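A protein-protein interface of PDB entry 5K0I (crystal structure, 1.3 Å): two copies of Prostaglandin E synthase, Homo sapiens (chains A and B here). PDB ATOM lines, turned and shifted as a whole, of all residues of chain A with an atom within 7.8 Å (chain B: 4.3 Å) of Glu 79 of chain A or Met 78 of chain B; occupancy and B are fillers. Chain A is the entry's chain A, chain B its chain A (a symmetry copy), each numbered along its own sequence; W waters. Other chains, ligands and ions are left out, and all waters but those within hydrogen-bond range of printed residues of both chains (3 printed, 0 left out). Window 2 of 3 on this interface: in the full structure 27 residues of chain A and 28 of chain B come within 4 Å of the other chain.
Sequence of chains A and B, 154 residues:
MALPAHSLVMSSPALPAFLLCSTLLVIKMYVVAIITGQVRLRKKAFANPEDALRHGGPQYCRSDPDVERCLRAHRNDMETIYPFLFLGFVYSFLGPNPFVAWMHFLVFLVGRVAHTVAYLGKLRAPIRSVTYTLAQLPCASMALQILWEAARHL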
ATOM      1  N   MET A  29     -20.813  16.708   9.218  1.00  0.00           N
ATOM      2  CA  MET A  29     -21.432  16.811  10.544  1.00  0.00           C
ATOM      3  C   MET A  29     -22.299  18.067  10.646  1.00  0.00           C
ATOM      4  O   MET A  29     -23.413  18.024  11.175  1.00  0.00           O
ATOM      5  CB  MET A  29     -20.369  16.778  11.641  1.00  0.00           C
ATOM      6  CG  MET A  29     -19.571  15.482  11.631  1.00  0.00           C
ATOM      7  SD  MET A  29     -18.452  15.292  13.032  1.00  0.00           S
ATOM      8  CE  MET A  29     -19.626  15.393  14.388  1.00  0.00           C
ATOM      9  N   ARG A  72     -29.177  10.669  16.836  1.00  0.00           N
ATOM     10  CA  ARG A  72     -28.381   9.440  16.885  1.00  0.00           C
ATOM     11  C   ARG A  72     -27.279   9.444  15.846  1.00  0.00           C
ATOM     12  O   ARG A  72     -26.154   9.039  16.141  1.00  0.00           O
ATOM     13  CB  ARG A  72     -29.253   8.187  16.705  1.00  0.00           C
ATOM     14  CG  ARG A  72     -30.175   7.900  17.879  1.00  0.00           C
ATOM     15  CD  ARG A  72     -30.727   6.475  17.866  1.00  0.00           C
ATOM     16  NE  ARG A  72     -31.643   6.206  16.757  1.00  0.00           N
ATOM     17  CZ  ARG A  72     -32.928   6.548  16.739  1.00  0.00           C
ATOM     18  NH1 ARG A  72     -33.450   7.204  17.765  1.00  0.00           N
ATOM     19  NH2 ARG A  72     -33.682   6.231  15.688  1.00  0.00           N
ATOM     20  N   ALA A  73     -27.591   9.895  14.630  1.00  0.00           N
ATOM     21  CA  ALA A  73     -26.580   9.952  13.581  1.00  0.00           C
ATOM     22  C   ALA A  73     -25.472  10.932  13.976  1.00  0.00           C
ATOM     23  O   ALA A  73     -24.283  10.646  13.806  1.00  0.00           O
ATOM     24  CB  ALA A  73     -27.205  10.352  12.255  1.00  0.00           C
ATOM     25  N   HIS A  74     -25.868  12.086  14.513  1.00  0.00           N
ATOM     26  CA  HIS A  74     -24.900  13.099  14.936  1.00  0.00           C
ATOM     27  C   HIS A  74     -24.045  12.574  16.093  1.00  0.00           C
ATOM     28  O   HIS A  74     -22.809  12.770  16.113  1.00  0.00           O
ATOM     29  CB  HIS A  74     -25.634  14.373  15.337  1.00  0.00           C
ATOM     30  CG  HIS A  74     -24.800  15.614  15.229  1.00  0.00           C
ATOM     31  ND1 HIS A  74     -25.357  16.875  15.291  1.00  0.00           N
ATOM     32  CD2 HIS A  74     -23.464  15.794  15.079  1.00  0.00           C
ATOM     33  CE1 HIS A  74     -24.397  17.779  15.176  1.00  0.00           C
ATOM     34  NE2 HIS A  74     -23.241  17.151  15.040  1.00  0.00           N
ATOM     35  N   ARG A  75     -24.671  11.893  17.052  1.00  0.00           N
ATOM     36  CA  ARG A  75     -23.918  11.307  18.151  1.00  0.00           C
ATOM     37  C   ARG A  75     -22.935  10.248  17.650  1.00  0.00           C
ATOM     38  O   ARG A  75     -21.768  10.219  18.074  1.00  0.00           O
ATOM     39  CB  ARG A  75     -24.855  10.731  19.208  1.00  0.00           C
ATOM     40  CG  ARG A  75     -24.100  10.233  20.403  1.00  0.00           C
ATOM     41  CD  ARG A  75     -24.995   9.662  21.460  1.00  0.00           C
ATOM     42  NE  ARG A  75     -24.145   8.925  22.374  1.00  0.00           N
ATOM     43  CZ  ARG A  75     -24.322   8.819  23.687  1.00  0.00           C
ATOM     44  NH1 ARG A  75     -23.437   8.125  24.357  1.00  0.00           N
ATOM     45  NH2 ARG A  75     -25.342   9.405  24.325  1.00  0.00           N
ATOM     46  N   ASN A  76     -23.383   9.386  16.736  1.00  0.00           N
ATOM     47  CA  ASN A  76     -22.492   8.368  16.202  1.00  0.00           C
ATOM     48  C   ASN A  76     -21.302   9.001  15.478  1.00  0.00           C
ATOM     49  O   ASN A  76     -20.171   8.526  15.613  1.00  0.00           O
ATOM     50  CB  ASN A  76     -23.275   7.393  15.314  1.00  0.00           C
ATOM     51  CG  ASN A  76     -22.469   6.167  14.967  1.00  0.00           C
ATOM     52  OD1 ASN A  76     -21.638   6.194  14.057  1.00  0.00           O
ATOM     53  ND2 ASN A  76     -22.680   5.085  15.718  1.00  0.00           N
ATOM     54  N   ASP A  77     -21.558  10.075  14.734  1.00  0.00           N
ATOM     55  CA  ASP A  77     -20.486  10.882  14.165  1.00  0.00           C
ATOM     56  C   ASP A  77     -19.478  11.344  15.236  1.00  0.00           C
ATOM     57  O   ASP A  77     -18.266  11.248  15.043  1.00  0.00           O
ATOM     58  CB  ASP A  77     -21.058  12.133  13.505  1.00  0.00           C
ATOM     59  CG  ASP A  77     -21.713  11.885  12.154  1.00  0.00           C
ATOM     60  OD1 ASP A  77     -21.750  10.739  11.648  1.00  0.00           O
ATOM     61  OD2 ASP A  77     -22.217  12.888  11.603  1.00  0.00           O
ATOM     62  N   MET A  78     -19.967  11.855  16.365  1.00  0.00           N
ATOM     63  CA  MET A  78     -19.060  12.306  17.424  1.00  0.00           C
ATOM     64  C   MET A  78     -18.261  11.148  18.034  1.00  0.00           C
ATOM     65  O   MET A  78     -17.106  11.338  18.440  1.00  0.00           O
ATOM     66  CB  MET A  78     -19.822  13.056  18.519  1.00  0.00           C
ATOM     67  CG  MET A  78     -20.509  14.332  18.024  1.00  0.00           C
ATOM     68  SD  MET A  78     -20.994  15.454  19.341  1.00  0.00           S
ATOM     69  CE  MET A  78     -22.190  14.491  20.231  1.00  0.00           C
ATOM     70  N   GLU A  79     -18.862   9.955  18.065  1.00  0.00           N
ATOM     71  CA  GLU A  79     -18.199   8.748  18.574  1.00  0.00           C
ATOM     72  C   GLU A  79     -17.077   8.241  17.653  1.00  0.00           C
ATOM     73  O   GLU A  79     -16.227   7.454  18.083  1.00  0.00           O
ATOM     74  CB  GLU A  79     -19.236   7.638  18.815  1.00  0.00           C
ATOM     75  CG  GLU A  79     -20.209   7.977  19.951  1.00  0.00           C
ATOM     76  CD  GLU A  79     -21.386   7.016  20.073  1.00  0.00           C
ATOM     77  OE1 GLU A  79     -21.479   6.036  19.297  1.00  0.00           O
ATOM     78  OE2 GLU A  79     -22.246   7.258  20.951  1.00  0.00           O
ATOM     79  N   THR A  80     -17.065   8.682  16.393  1.00  0.00           N
ATOM     80  CA  THR A  80     -16.170   8.083  15.398  1.00  0.00           C
ATOM     81  C   THR A  80     -15.312   9.096  14.646  1.00  0.00           C
ATOM     82  O   THR A  80     -14.109   8.878  14.458  1.00  0.00           O
ATOM     83  CB  THR A  80     -16.959   7.246  14.363  1.00  0.00           C
ATOM     84  OG1 THR A  80     -17.963   8.070  13.751  1.00  0.00           O
ATOM     85  CG2 THR A  80     -17.595   6.031  15.023  1.00  0.00           C
ATOM     86  N   ILE A  81     -15.927  10.182  14.185  1.00  0.00           N
ATOM     87  CA  ILE A  81     -15.194  11.184  13.399  1.00  0.00           C
ATOM     88  C   ILE A  81     -14.192  11.950  14.267  1.00  0.00           C
ATOM     89  O   ILE A  81     -13.064  12.221  13.837  1.00  0.00           O
ATOM     90  CB  ILE A  81     -16.155  12.118  12.620  1.00  0.00           C
ATOM     91  CG1 ILE A  81     -16.947  11.282  11.596  1.00  0.00           C
ATOM     92  CG2 ILE A  81     -15.381  13.265  11.962  1.00  0.00           C
ATOM     93  CD1 ILE A  81     -18.087  12.011  10.914  1.00  0.00           C
ATOM     94  N   TYR A  82     -14.579  12.281  15.500  1.00  0.00           N
ATOM     95  CA  TYR A  82     -13.643  12.981  16.387  1.00  0.00           C
ATOM     96  C   TYR A  82     -12.365  12.152  16.648  1.00  0.00           C
ATOM     97  O   TYR A  82     -11.256  12.678  16.510  1.00  0.00           O
ATOM     98  CB  TYR A  82     -14.319  13.485  17.669  1.00  0.00           C
ATOM     99  CG  TYR A  82     -15.417  14.522  17.460  1.00  0.00           C
ATOM    100  CD1 TYR A  82     -15.520  15.277  16.287  1.00  0.00           C
ATOM    101  CD2 TYR A  82     -16.352  14.761  18.468  1.00  0.00           C
ATOM    102  CE1 TYR A  82     -16.536  16.230  16.133  1.00  0.00           C
ATOM    103  CE2 TYR A  82     -17.351  15.704  18.320  1.00  0.00           C
ATOM    104  CZ  TYR A  82     -17.434  16.441  17.158  1.00  0.00           C
ATOM    105  OH  TYR A  82     -18.433  17.380  17.003  1.00  0.00           O
ATOM    106  N   PRO A  83     -12.489  10.847  16.983  1.00  0.00           N
ATOM    107  CA  PRO A  83     -11.263  10.025  17.072  1.00  0.00           C
ATOM    108  C   PRO A  83     -10.433  10.016  15.781  1.00  0.00           C
ATOM    109  O   PRO A  83      -9.204  10.076  15.848  1.00  0.00           O
ATOM    110  CB  PRO A  83     -11.803   8.627  17.375  1.00  0.00           C
ATOM    111  CG  PRO A  83     -13.063   8.891  18.126  1.00  0.00           C
ATOM    112  CD  PRO A  83     -13.657  10.137  17.532  1.00  0.00           C
ATOM    113  N   PHE A  84     -11.082   9.967  14.620  1.00  0.00           N
ATOM    114  CA  PHE A  84     -10.374  10.023  13.341  1.00  0.00           C
ATOM    115  C   PHE A  84      -9.570  11.310  13.169  1.00  0.00           C
ATOM    116  O   PHE A  84      -8.450  11.284  12.638  1.00  0.00           O
ATOM    117  CB  PHE A  84     -11.357   9.871  12.186  1.00  0.00           C
ATOM    118  CG  PHE A  84     -10.725  10.043  10.822  1.00  0.00           C
ATOM    119  CD1 PHE A  84     -10.081   8.976  10.192  1.00  0.00           C
ATOM    120  CD2 PHE A  84     -10.788  11.267  10.169  1.00  0.00           C
ATOM    121  CE1 PHE A  84      -9.509   9.135   8.925  1.00  0.00           C
ATOM    122  CE2 PHE A  84     -10.209  11.434   8.907  1.00  0.00           C
ATOM    123  CZ  PHE A  84      -9.574  10.366   8.286  1.00  0.00           C
ATOM    124  N   PHE A 108     -12.434   5.726   5.267  1.00  0.00           N
ATOM    125  CA  PHE A 108     -13.157   6.369   6.364  1.00  0.00           C
ATOM    126  C   PHE A 108     -14.181   7.381   5.843  1.00  0.00           C
ATOM    127  O   PHE A 108     -15.334   7.376   6.267  1.00  0.00           O
ATOM    128  CB  PHE A 108     -12.213   7.030   7.373  1.00  0.00           C
ATOM    129  CG  PHE A 108     -12.931   7.472   8.622  1.00  0.00           C
ATOM    130  CD1 PHE A 108     -13.397   6.526   9.539  1.00  0.00           C
ATOM    131  CD2 PHE A 108     -13.200   8.821   8.858  1.00  0.00           C
ATOM    132  CE1 PHE A 108     -14.100   6.917  10.678  1.00  0.00           C
ATOM    133  CE2 PHE A 108     -13.905   9.219  10.000  1.00  0.00           C
ATOM    134  CZ  PHE A 108     -14.344   8.266  10.915  1.00  0.00           C
ATOM    135  N   ARG A 112     -18.171   6.740   6.259  1.00  0.00           N
ATOM    136  CA  ARG A 112     -18.938   7.664   7.106  1.00  0.00           C
ATOM    137  C   ARG A 112     -20.048   8.410   6.353  1.00  0.00           C
ATOM    138  O   ARG A 112     -21.149   8.600   6.884  1.00  0.00           O
ATOM    139  CB  ARG A 112     -18.002   8.640   7.826  1.00  0.00           C
ATOM    140  CG  ARG A 112     -17.144   7.999   8.917  1.00  0.00           C
ATOM    141  CD  ARG A 112     -17.926   7.113   9.901  1.00  0.00           C
ATOM    142  NE  ARG A 112     -19.036   7.819  10.553  1.00  0.00           N
ATOM    143  CZ  ARG A 112     -19.802   7.283  11.502  1.00  0.00           C
ATOM    144  NH1 ARG A 112     -19.581   6.039  11.908  1.00  0.00           N
ATOM    145  NH2 ARG A 112     -20.784   7.988  12.055  1.00  0.00           N
ATOM    146  N   TYR A 132     -20.591   1.308   9.104  1.00  0.00           N
ATOM    147  CA  TYR A 132     -19.916   1.659  10.354  1.00  0.00           C
ATOM    148  C   TYR A 132     -18.634   0.835  10.506  1.00  0.00           C
ATOM    149  O   TYR A 132     -17.553   1.371  10.792  1.00  0.00           O
ATOM    150  CB  TYR A 132     -20.843   1.409  11.559  1.00  0.00           C
ATOM    151  CG  TYR A 132     -20.186   1.785  12.864  1.00  0.00           C
ATOM    152  CD1 TYR A 132     -19.356   0.886  13.538  1.00  0.00           C
ATOM    153  CD2 TYR A 132     -20.356   3.061  13.405  1.00  0.00           C
ATOM    154  CE1 TYR A 132     -18.721   1.250  14.725  1.00  0.00           C
ATOM    155  CE2 TYR A 132     -19.731   3.434  14.589  1.00  0.00           C
ATOM    156  CZ  TYR A 132     -18.915   2.523  15.244  1.00  0.00           C
ATOM    157  OH  TYR A 132     -18.291   2.886  16.414  1.00  0.00           O
ATOM    158  N   GLN A 136     -14.569   1.929  10.517  1.00  0.00           N
ATOM    159  CA  GLN A 136     -13.727   1.732  11.691  1.00  0.00           C
ATOM    160  C   GLN A 136     -12.433   0.979  11.396  1.00  0.00           C
ATOM    161  O   GLN A 136     -11.470   1.137  12.130  1.00  0.00           O
ATOM    162  CB  GLN A 136     -14.486   1.043  12.831  1.00  0.00           C
ATOM    163  CG  GLN A 136     -15.549   1.910  13.501  1.00  0.00           C
ATOM    164  CD  GLN A 136     -15.020   3.274  13.921  1.00  0.00           C
ATOM    165  OE1 GLN A 136     -15.171   4.251  13.198  1.00  0.00           O
ATOM    166  NE2 GLN A 136     -14.367   3.331  15.078  1.00  0.00           N
ATOM    167  N   MET B  29     -12.356   3.795  24.215  1.00  0.00           N
ATOM    168  CA  MET B  29     -13.662   4.280  23.753  1.00  0.00           C
ATOM    169  C   MET B  29     -14.275   3.314  22.739  1.00  0.00           C
ATOM    170  O   MET B  29     -15.469   3.013  22.796  1.00  0.00           O
ATOM    171  CB  MET B  29     -13.542   5.690  23.180  1.00  0.00           C
ATOM    172  CG  MET B  29     -13.044   6.692  24.211  1.00  0.00           C
ATOM    173  SD  MET B  29     -13.089   8.407  23.657  1.00  0.00           S
ATOM    174  CE  MET B  29     -14.840   8.574  23.292  1.00  0.00           C
ATOM    175  N   HIS B  74     -20.025   6.177  27.450  1.00  0.00           N
ATOM    176  CA  HIS B  74     -19.454   6.649  26.188  1.00  0.00           C
ATOM    177  C   HIS B  74     -19.578   8.171  26.080  1.00  0.00           C
ATOM    178  O   HIS B  74     -18.624   8.861  25.658  1.00  0.00           O
ATOM    179  CB  HIS B  74     -20.153   5.962  25.021  1.00  0.00           C
ATOM    180  CG  HIS B  74     -19.328   5.898  23.771  1.00  0.00           C
ATOM    181  ND1 HIS B  74     -19.677   5.094  22.706  1.00  0.00           N
ATOM    182  CD2 HIS B  74     -18.189   6.540  23.408  1.00  0.00           C
ATOM    183  CE1 HIS B  74     -18.782   5.238  21.742  1.00  0.00           C
ATOM    184  NE2 HIS B  74     -17.866   6.104  22.143  1.00  0.00           N
ATOM    185  N   ARG B  75     -20.731   8.718  26.468  1.00  0.00           N
ATOM    186  CA  ARG B  75     -20.903  10.162  26.456  1.00  0.00           C
ATOM    187  C   ARG B  75     -19.929  10.848  27.416  1.00  0.00           C
ATOM    188  O   ARG B  75     -19.303  11.860  27.064  1.00  0.00           O
ATOM    189  CB  ARG B  75     -22.346  10.542  26.772  1.00  0.00           C
ATOM    190  CG  ARG B  75     -22.569  12.019  26.643  1.00  0.00           C
ATOM    191  CD  ARG B  75     -23.979  12.423  26.948  1.00  0.00           C
ATOM    192  NE  ARG B  75     -23.974  13.862  27.122  1.00  0.00           N
ATOM    193  CZ  ARG B  75     -24.951  14.692  26.772  1.00  0.00           C
ATOM    194  NH1 ARG B  75     -24.760  15.968  26.989  1.00  0.00           N
ATOM    195  NH2 ARG B  75     -26.084  14.268  26.199  1.00  0.00           N
ATOM    196  N   ASN B  76     -19.775  10.297  28.621  1.00  0.00           N
ATOM    197  CA  ASN B  76     -18.848  10.886  29.574  1.00  0.00           C
ATOM    198  C   ASN B  76     -17.415  10.865  29.036  1.00  0.00           C
ATOM    199  O   ASN B  76     -16.677  11.839  29.202  1.00  0.00           O
ATOM    200  CB  ASN B  76     -18.978  10.195  30.937  1.00  0.00           C
ATOM    201  CG  ASN B  76     -18.253  10.944  32.027  1.00  0.00           C
ATOM    202  OD1 ASN B  76     -17.037  10.820  32.176  1.00  0.00           O
ATOM    203  ND2 ASN B  76     -18.992  11.762  32.777  1.00  0.00           N
ATOM    204  N   ASP B  77     -17.041   9.770  28.378  1.00  0.00           N
ATOM    205  CA  ASP B  77     -15.781   9.712  27.647  1.00  0.00           C
ATOM    206  C   ASP B  77     -15.642  10.872  26.642  1.00  0.00           C
ATOM    207  O   ASP B  77     -14.597  11.519  26.568  1.00  0.00           O
ATOM    208  CB  ASP B  77     -15.686   8.409  26.858  1.00  0.00           C
ATOM    209  CG  ASP B  77     -15.357   7.186  27.704  1.00  0.00           C
ATOM    210  OD1 ASP B  77     -15.172   7.280  28.939  1.00  0.00           O
ATOM    211  OD2 ASP B  77     -15.302   6.100  27.088  1.00  0.00           O
ATOM    212  N   MET B  78     -16.685  11.137  25.856  1.00  0.00           N
ATOM    213  CA  MET B  78     -16.616  12.232  24.884  1.00  0.00           C
ATOM    214  C   MET B  78     -16.496  13.603  25.564  1.00  0.00           C
ATOM    215  O   MET B  78     -15.848  14.508  25.022  1.00  0.00           O
ATOM    216  CB  MET B  78     -17.824  12.212  23.946  1.00  0.00           C
ATOM    217  CG  MET B  78     -17.919  10.941  23.096  1.00  0.00           C
ATOM    218  SD  MET B  78     -19.021  11.092  21.685  1.00  0.00           S
ATOM    219  CE  MET B  78     -20.594  11.356  22.464  1.00  0.00           C
ATOM    220  N   GLU B  79     -17.090  13.736  26.754  1.00  0.00           N
ATOM    221  CA  GLU B  79     -17.015  14.974  27.539  1.00  0.00           C
ATOM    222  C   GLU B  79     -15.617  15.235  28.125  1.00  0.00           C
ATOM    223  O   GLU B  79     -15.310  16.363  28.522  1.00  0.00           O
ATOM    224  CB  GLU B  79     -18.068  14.951  28.660  1.00  0.00           C
ATOM    225  CG  GLU B  79     -19.504  14.995  28.121  1.00  0.00           C
ATOM    226  CD  GLU B  79     -20.575  14.746  29.177  1.00  0.00           C
ATOM    227  OE1 GLU B  79     -20.247  14.554  30.371  1.00  0.00           O
ATOM    228  OE2 GLU B  79     -21.769  14.722  28.798  1.00  0.00           O
ATOM    229  N   THR B  80     -14.769  14.206  28.182  1.00  0.00           N
ATOM    230  CA  THR B  80     -13.508  14.314  28.922  1.00  0.00           C
ATOM    231  C   THR B  80     -12.278  13.919  28.110  1.00  0.00           C
ATOM    232  O   THR B  80     -11.255  14.613  28.147  1.00  0.00           O
ATOM    233  CB  THR B  80     -13.537  13.463  30.212  1.00  0.00           C
ATOM    234  OG1 THR B  80     -13.844  12.102  29.878  1.00  0.00           O
ATOM    235  CG2 THR B  80     -14.557  14.014  31.200  1.00  0.00           C
ATOM    236  N   TYR B  82     -11.957  13.667  24.756  1.00  0.00           N
ATOM    237  CA  TYR B  82     -11.734  14.563  23.615  1.00  0.00           C
ATOM    238  C   TYR B  82     -10.995  15.855  24.030  1.00  0.00           C
ATOM    239  O   TYR B  82     -10.006  16.226  23.390  1.00  0.00           O
ATOM    240  CB  TYR B  82     -13.019  14.822  22.816  1.00  0.00           C
ATOM    241  CG  TYR B  82     -13.633  13.592  22.158  1.00  0.00           C
ATOM    242  CD1 TYR B  82     -12.899  12.424  21.919  1.00  0.00           C
ATOM    243  CD2 TYR B  82     -14.967  13.610  21.749  1.00  0.00           C
ATOM    244  CE1 TYR B  82     -13.493  11.315  21.302  1.00  0.00           C
ATOM    245  CE2 TYR B  82     -15.552  12.521  21.135  1.00  0.00           C
ATOM    246  CZ  TYR B  82     -14.812  11.381  20.905  1.00  0.00           C
ATOM    247  OH  TYR B  82     -15.393  10.288  20.297  1.00  0.00           O
ATOM    248  N   PRO B  83     -11.424  16.533  25.120  1.00  0.00           N
ATOM    249  CA  PRO B  83     -10.616  17.673  25.602  1.00  0.00           C
ATOM    250  C   PRO B  83      -9.161  17.303  25.925  1.00  0.00           C
ATOM    251  O   PRO B  83      -8.254  18.075  25.611  1.00  0.00           O
ATOM    252  CB  PRO B  83     -11.354  18.112  26.868  1.00  0.00           C
ATOM    253  CG  PRO B  83     -12.772  17.749  26.592  1.00  0.00           C
ATOM    254  CD  PRO B  83     -12.736  16.478  25.789  1.00  0.00           C
HETATM  255  O   HOH W   1     -21.518   8.653  22.983  1.00  0.00           O
HETATM  256  O   HOH W   2     -15.608   7.309  20.690  1.00  0.00           O
HETATM  257  O   HOH W   3     -26.186  12.293  23.889  1.00  0.00           O
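Arg 75 of chain A touches His 74 of chain B. Glu 79 of chain A touches His 74 of chain B. Tyr 82 of chain B touches Glu 79 of chain A (OH to CA, 3.6 Å). Tyr 82 of chain A touches Tyr 82 of chain B. CD of Pro 83 of chain A touches OH of Tyr 82 of chain B, at 3.3 Å.
O of Met 78 of chain A is in hydrogen-bond range of OH of Tyr 82 of chain B (2.7 Å). N of Glu 79 of chain A sits close to SD of Met 78 of chain B (3.8 Å). The guanidinium group (NH1) of Arg 75 of chain A sits close to the backbone NH (N) of Arg 75 of chain B (3.5 Å). The backbone carbonyl oxygen of Met 78 of chain A lies close to the side-chain sulfur of Met 78 of chain B (3.8 Å).
Water W1 lies within hydrogen-bond range of NH1 of Arg 75 of chain A (2.4 Å), OE2 of Glu 79 of chain A (2.6 Å) and SD of Met 78 of chain B (3.7 Å). Water W2 lies within hydrogen-bond range of the backbone carbonyl oxygen of Glu 79 of chain A (2.7 Å), a ring nitrogen (NE2) of His 74 of chain B (2.9 Å) and the side-chain hydroxyl of Tyr 82 of chain B (3.0 Å). Water W3 bridges NH2 of Arg 75 of chain A (3.0 Å) and NH2 of Arg 75 of chain B (3.0 Å).
Arg 75 of chain A touches His 74 of chain B, but with the chains exchanged His 74 of chain A does not touch Arg 75 of chain B (10.4 Å). Met 78 of chain B touches its own counterpart, Met 78 of chain A. Glu 79 of chain A touches Met 78 of chain B, but with the chains exchanged Met 78 of chain A does not touch Glu 79 of chain B (8.3 Å). Glu 79 of chain A touches Tyr 82 of chain B, but with the chains exchanged Tyr 82 of chain A does not touch Glu 79 of chain B (8.4 Å). Of the 9 pairs that touch across the chains among the printed residues, 3 have their exchanged pair printed and touching as well.
Hydrophobic or aromatic side chains of chain B that line the printed part of chain A: His 74, Met 78 and Tyr 82. Printed residues of chain A that touch a printed residue of chain B: Arg 75, Met 78, Glu 79, Tyr 82 and Pro 83. Hydrophobic or aromatic side chains of chain A that line the printed part of chain B: Met 78, Tyr 82 and Pro 83.
The side-chain carboxylate (OE2) of Glu 79 of chain A lies within salt-bridge range of the guanidinium group (NE) of Arg 75 of chain A (2.9 Å). The guanidinium group (NE) of Arg 75 of chain B is in salt-bridge range of the side-chain carboxylate (OE2) of Glu 79 of chain B (2.9 Å).
Glu 79 of chain A touches just these residues of chain B: His 74, Met 78 and Tyr 82. Printed residues of chain B within 4 Å of Met 78 of chain A: Met 78 (3.7 Å) and Tyr 82 (2.7 Å). Of the printed residues of chain A, Arg 75 of chain B touches Arg 75. Of the printed residues of chain B, Tyr 82 of chain A touches Tyr 82 (3.6 Å). Asn 76 of chain B touches none of the printed residues of chain A. The nearest printed residue of chain B that does not touch Glu 79 of chain A is Met 29 of chain B (5.5 Å). The nearest printed residue of chain A that does not touch Met 78 of chain B is Arg 75 of chain A (4.2 Å).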
